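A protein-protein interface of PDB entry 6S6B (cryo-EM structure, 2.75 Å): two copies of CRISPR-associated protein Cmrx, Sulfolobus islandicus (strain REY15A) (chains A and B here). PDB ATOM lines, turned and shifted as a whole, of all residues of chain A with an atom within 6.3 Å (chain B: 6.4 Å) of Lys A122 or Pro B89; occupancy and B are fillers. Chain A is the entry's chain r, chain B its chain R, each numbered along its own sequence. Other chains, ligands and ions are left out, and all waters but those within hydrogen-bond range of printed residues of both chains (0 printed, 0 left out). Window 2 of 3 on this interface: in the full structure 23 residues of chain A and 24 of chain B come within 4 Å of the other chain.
No position is printed for both chains.
Of the printed residues of chain B, Lys A122 touches Pro B89 (3.3 Å) and Lys B92 (3.6 Å).
Of the printed residues of chain A, Pro B89 touches Ser A120, Met A121 and Lys A122.
Printed residues of chain A within 4 Å of Asp B105: Ser A120.
Printed residues of chain A within 4 Å of Leu B88: Ser A120 (3.7 Å) and Met A121 (3.8 Å).
Of the printed residues of chain A, Lys B92 touches Lys A122 and Thr A123.
Printed residues of chain B within 4 Å of Met A121: Lys B87 (3.0 Å), Leu B88 (3.8 Å) and Pro B89 (3.99 Å).
Printed residues of chain B within 4 Å of Thr A123: Lys B92.
Lys A124 touches none of the printed residues of chain B.
The nearest printed residue of chain A that does not touch Pro B89 is Thr A123 (6.1 Å).
The nearest printed residue of chain A that does not touch Leu B88 is Lys A122 (5.4 Å).
Among the printed residues, merely in contact across the chains: Ser A120 with Asp B105, Lys A122 with Pro B89, Ser A120 with Lys B87, Lys A122 with Lys B92, Ser A120 with Leu B88, Met A121 with Leu B88, Ser A120 with Pro B89 and Met A121 with Pro B89.
N of Met A121 lies within hydrogen-bond range of O of Lys B87, 3.0 Å away.
The backbone carbonyl oxygen (O) of Thr A123 lies within hydrogen-bond range of the side-chain amino group (NZ) of Lys B92 (2.7 Å).
Of the 11 printed residues of chain B, 5 touch a printed residue of chain A.
Hydrophobic or aromatic side chains of chain B within 4 Å of the printed part of chain A: Pro B89.
Among the printed residues, no Asp or Glu carboxylate lies within 4 Å of a Lys or Arg side-chain nitrogen of the other chain.
The backbone carbonyl oxygen of Leu B88 sits at hydrogen-bond distance from the backbone NH of Leu B106 (2.6 Å).
O of Ala A171 is in hydrogen-bond range of OG1 of Thr A123 (2.6 Å).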
ATOM      1  N   SER A 120      22.163  -7.714  12.010  1.00  0.00           N
ATOM      2  CA  SER A 120      21.556  -9.031  12.076  1.00  0.00           C
ATOM      3  C   SER A 120      22.463  -9.935  12.896  1.00  0.00           C
ATOM      4  O   SER A 120      23.689  -9.875  12.774  1.00  0.00           O
ATOM      5  CB  SER A 120      21.335  -9.600  10.678  1.00  0.00           C
ATOM      6  OG  SER A 120      20.385  -8.820   9.980  1.00  0.00           O
ATOM      7  N   MET A 121      21.852 -10.749  13.757  1.00  0.00           N
ATOM      8  CA  MET A 121      22.603 -11.466  14.782  1.00  0.00           C
ATOM      9  C   MET A 121      23.789 -12.218  14.187  1.00  0.00           C
ATOM     10  O   MET A 121      24.947 -11.893  14.469  1.00  0.00           O
ATOM     11  CB  MET A 121      21.670 -12.416  15.531  1.00  0.00           C
ATOM     12  CG  MET A 121      20.607 -11.708  16.351  1.00  0.00           C
ATOM     13  SD  MET A 121      21.234 -11.055  17.908  1.00  0.00           S
ATOM     14  CE  MET A 121      19.874  -9.993  18.384  1.00  0.00           C
ATOM     15  N   LYS A 122      23.516 -13.198  13.327  1.00  0.00           N
ATOM     16  CA  LYS A 122      24.552 -13.994  12.672  1.00  0.00           C
ATOM     17  C   LYS A 122      25.539 -14.552  13.699  1.00  0.00           C
ATOM     18  O   LYS A 122      26.736 -14.264  13.685  1.00  0.00           O
ATOM     19  CB  LYS A 122      25.275 -13.177  11.598  1.00  0.00           C
ATOM     20  CG  LYS A 122      26.083 -14.014  10.617  1.00  0.00           C
ATOM     21  CD  LYS A 122      26.454 -13.217   9.378  1.00  0.00           C
ATOM     22  CE  LYS A 122      25.244 -12.497   8.800  1.00  0.00           C
ATOM     23  NZ  LYS A 122      24.118 -13.431   8.522  1.00  0.00           N
ATOM     24  N   THR A 123      24.999 -15.347  14.609  1.00  0.00           N
ATOM     25  CA  THR A 123      25.783 -15.985  15.651  1.00  0.00           C
ATOM     26  C   THR A 123      26.290 -17.348  15.196  1.00  0.00           C
ATOM     27  O   THR A 123      25.684 -18.011  14.350  1.00  0.00           O
ATOM     28  CB  THR A 123      24.954 -16.130  16.924  1.00  0.00           C
ATOM     29  OG1 THR A 123      25.717 -16.815  17.924  1.00  0.00           O
ATOM     30  CG2 THR A 123      23.675 -16.872  16.639  1.00  0.00           C
ATOM     31  N   LYS A 124      27.415 -17.759  15.772  1.00  0.00           N
ATOM     32  CA  LYS A 124      28.092 -18.986  15.397  1.00  0.00           C
ATOM     33  C   LYS A 124      28.555 -19.705  16.654  1.00  0.00           C
ATOM     34  O   LYS A 124      28.866 -19.059  17.661  1.00  0.00           O
ATOM     35  CB  LYS A 124      29.296 -18.705  14.484  1.00  0.00           C
ATOM     36  CG  LYS A 124      29.001 -17.787  13.309  1.00  0.00           C
ATOM     37  CD  LYS A 124      30.181 -16.883  13.007  1.00  0.00           C
ATOM     38  CE  LYS A 124      29.761 -15.696  12.168  1.00  0.00           C
ATOM     39  NZ  LYS A 124      30.738 -14.583  12.268  1.00  0.00           N
ATOM     40  N   ALA A 171      27.870 -17.199  20.077  1.00  0.00           N
ATOM     41  CA  ALA A 171      28.229 -15.792  20.109  1.00  0.00           C
ATOM     42  C   ALA A 171      28.040 -15.190  18.727  1.00  0.00           C
ATOM     43  O   ALA A 171      28.146 -15.886  17.715  1.00  0.00           O
ATOM     44  CB  ALA A 171      29.671 -15.592  20.576  1.00  0.00           C
ATOM     45  N   LEU A 172      27.761 -13.884  18.697  1.00  0.00           N
ATOM     46  CA  LEU A 172      27.590 -13.196  17.423  1.00  0.00           C
ATOM     47  C   LEU A 172      28.888 -13.152  16.633  1.00  0.00           C
ATOM     48  O   LEU A 172      28.858 -13.043  15.402  1.00  0.00           O
ATOM     49  CB  LEU A 172      27.065 -11.778  17.644  1.00  0.00           C
ATOM     50  CG  LEU A 172      25.644 -11.627  18.188  1.00  0.00           C
ATOM     51  CD1 LEU A 172      25.139 -10.200  18.031  1.00  0.00           C
ATOM     52  CD2 LEU A 172      24.706 -12.603  17.533  1.00  0.00           C
ATOM     53  N   GLU A 173      30.029 -13.225  17.319  1.00  0.00           N
ATOM     54  CA  GLU A 173      31.347 -13.262  16.685  1.00  0.00           C
ATOM     55  C   GLU A 173      31.579 -12.017  15.828  1.00  0.00           C
ATOM     56  O   GLU A 173      31.877 -12.091  14.635  1.00  0.00           O
ATOM     57  CB  GLU A 173      31.523 -14.545  15.866  1.00  0.00           C
ATOM     58  CG  GLU A 173      31.245 -15.811  16.654  1.00  0.00           C
ATOM     59  CD  GLU A 173      31.892 -17.032  16.045  1.00  0.00           C
ATOM     60  OE1 GLU A 173      32.735 -16.875  15.139  1.00  0.00           O
ATOM     61  OE2 GLU A 173      31.556 -18.153  16.472  1.00  0.00           O
ATOM     62  N   LYS B  87      17.178  -7.791  14.794  1.00  0.00           N
ATOM     63  CA  LYS B  87      17.575  -8.063  13.420  1.00  0.00           C
ATOM     64  C   LYS B  87      18.255  -9.422  13.364  1.00  0.00           C
ATOM     65  O   LYS B  87      19.090  -9.739  14.216  1.00  0.00           O
ATOM     66  CB  LYS B  87      18.531  -6.990  12.892  1.00  0.00           C
ATOM     67  CG  LYS B  87      17.941  -5.593  12.839  1.00  0.00           C
ATOM     68  CD  LYS B  87      18.997  -4.545  12.521  1.00  0.00           C
ATOM     69  CE  LYS B  87      19.422  -4.609  11.065  1.00  0.00           C
ATOM     70  NZ  LYS B  87      20.403  -3.540  10.720  1.00  0.00           N
ATOM     71  N   LEU B  88      17.904 -10.221  12.361  1.00  0.00           N
ATOM     72  CA  LEU B  88      18.485 -11.547  12.210  1.00  0.00           C
ATOM     73  C   LEU B  88      18.405 -11.968  10.752  1.00  0.00           C
ATOM     74  O   LEU B  88      17.508 -11.521  10.027  1.00  0.00           O
ATOM     75  CB  LEU B  88      17.783 -12.570  13.114  1.00  0.00           C
ATOM     76  CG  LEU B  88      16.263 -12.690  13.050  1.00  0.00           C
ATOM     77  CD1 LEU B  88      15.837 -13.594  11.921  1.00  0.00           C
ATOM     78  CD2 LEU B  88      15.729 -13.222  14.365  1.00  0.00           C
ATOM     79  N   PRO B  89      19.318 -12.831  10.293  1.00  0.00           N
ATOM     80  CA  PRO B  89      19.408 -13.137   8.858  1.00  0.00           C
ATOM     81  C   PRO B  89      18.354 -14.097   8.323  1.00  0.00           C
ATOM     82  O   PRO B  89      18.536 -14.658   7.237  1.00  0.00           O
ATOM     83  CB  PRO B  89      20.808 -13.744   8.722  1.00  0.00           C
ATOM     84  CG  PRO B  89      21.121 -14.273  10.068  1.00  0.00           C
ATOM     85  CD  PRO B  89      20.487 -13.332  11.034  1.00  0.00           C
ATOM     86  N   ALA B  90      17.278 -14.326   9.075  1.00  0.00           N
ATOM     87  CA  ALA B  90      16.133 -15.160   8.706  1.00  0.00           C
ATOM     88  C   ALA B  90      16.478 -16.640   8.627  1.00  0.00           C
ATOM     89  O   ALA B  90      15.577 -17.461   8.414  1.00  0.00           O
ATOM     90  CB  ALA B  90      15.488 -14.736   7.381  1.00  0.00           C
ATOM     91  N   ASN B  91      17.744 -17.015   8.788  1.00  0.00           N
ATOM     92  CA  ASN B  91      18.118 -18.393   9.048  1.00  0.00           C
ATOM     93  C   ASN B  91      18.225 -18.670  10.535  1.00  0.00           C
ATOM     94  O   ASN B  91      18.830 -19.672  10.934  1.00  0.00           O
ATOM     95  CB  ASN B  91      19.438 -18.727   8.351  1.00  0.00           C
ATOM     96  CG  ASN B  91      19.232 -19.311   6.971  1.00  0.00           C
ATOM     97  OD1 ASN B  91      18.124 -19.706   6.613  1.00  0.00           O
ATOM     98  ND2 ASN B  91      20.302 -19.370   6.186  1.00  0.00           N
ATOM     99  N   LYS B  92      17.658 -17.793  11.365  1.00  0.00           N
ATOM    100  CA  LYS B  92      17.776 -17.925  12.810  1.00  0.00           C
ATOM    101  C   LYS B  92      16.451 -17.657  13.510  1.00  0.00           C
ATOM    102  O   LYS B  92      16.447 -17.201  14.658  1.00  0.00           O
ATOM    103  CB  LYS B  92      18.856 -16.989  13.349  1.00  0.00           C
ATOM    104  CG  LYS B  92      20.243 -17.390  12.906  1.00  0.00           C
ATOM    105  CD  LYS B  92      21.322 -16.633  13.635  1.00  0.00           C
ATOM    106  CE  LYS B  92      22.692 -17.067  13.142  1.00  0.00           C
ATOM    107  NZ  LYS B  92      23.123 -18.363  13.730  1.00  0.00           N
ATOM    108  N   ILE B 102      12.710 -17.748   2.602  1.00  0.00           N
ATOM    109  CA  ILE B 102      13.233 -16.419   2.890  1.00  0.00           C
ATOM    110  C   ILE B 102      14.731 -16.421   2.619  1.00  0.00           C
ATOM    111  O   ILE B 102      15.411 -17.441   2.777  1.00  0.00           O
ATOM    112  CB  ILE B 102      12.917 -16.008   4.341  1.00  0.00           C
ATOM    113  CG1 ILE B 102      11.437 -16.241   4.657  1.00  0.00           C
ATOM    114  CG2 ILE B 102      13.257 -14.553   4.566  1.00  0.00           C
ATOM    115  CD1 ILE B 102      11.173 -17.495   5.462  1.00  0.00           C
ATOM    116  N   SER B 103      15.260 -15.270   2.197  1.00  0.00           N
ATOM    117  CA  SER B 103      16.641 -15.195   1.745  1.00  0.00           C
ATOM    118  C   SER B 103      17.425 -14.002   2.278  1.00  0.00           C
ATOM    119  O   SER B 103      18.652 -13.983   2.121  1.00  0.00           O
ATOM    120  CB  SER B 103      16.689 -15.164   0.210  1.00  0.00           C
ATOM    121  OG  SER B 103      16.137 -16.349  -0.334  1.00  0.00           O
ATOM    122  N   ASP B 104      16.776 -13.019   2.895  1.00  0.00           N
ATOM    123  CA  ASP B 104      17.433 -11.802   3.344  1.00  0.00           C
ATOM    124  C   ASP B 104      17.408 -11.709   4.862  1.00  0.00           C
ATOM    125  O   ASP B 104      16.776 -12.510   5.549  1.00  0.00           O
ATOM    126  CB  ASP B 104      16.763 -10.566   2.735  1.00  0.00           C
ATOM    127  CG  ASP B 104      15.398 -10.292   3.334  1.00  0.00           C
ATOM    128  OD1 ASP B 104      14.580 -11.234   3.402  1.00  0.00           O
ATOM    129  OD2 ASP B 104      15.146  -9.138   3.743  1.00  0.00           O
ATOM    130  N   ASP B 105      18.116 -10.710   5.379  1.00  0.00           N
ATOM    131  CA  ASP B 105      18.051 -10.408   6.800  1.00  0.00           C
ATOM    132  C   ASP B 105      16.725  -9.738   7.132  1.00  0.00           C
ATOM    133  O   ASP B 105      16.209  -8.930   6.355  1.00  0.00           O
ATOM    134  CB  ASP B 105      19.214  -9.507   7.204  1.00  0.00           C
ATOM    135  CG  ASP B 105      20.555 -10.064   6.778  1.00  0.00           C
ATOM    136  OD1 ASP B 105      20.640 -11.281   6.518  1.00  0.00           O
ATOM    137  OD2 ASP B 105      21.525  -9.283   6.703  1.00  0.00           O
ATOM    138  N   LEU B 106      16.171 -10.072   8.294  1.00  0.00           N
ATOM    139  CA  LEU B 106      14.825  -9.640   8.668  1.00  0.00           C
ATOM    140  C   LEU B 106      14.868  -8.940  10.021  1.00  0.00           C
ATOM    141  O   LEU B 106      14.978  -9.591  11.065  1.00  0.00           O
ATOM    142  CB  LEU B 106      13.867 -10.822   8.692  1.00  0.00           C
ATOM    143  CG  LEU B 106      13.647 -11.506   7.344  1.00  0.00           C
ATOM    144  CD1 LEU B 106      12.527 -12.518   7.441  1.00  0.00           C
ATOM    145  CD2 LEU B 106      13.354 -10.478   6.266  1.00  0.00           C
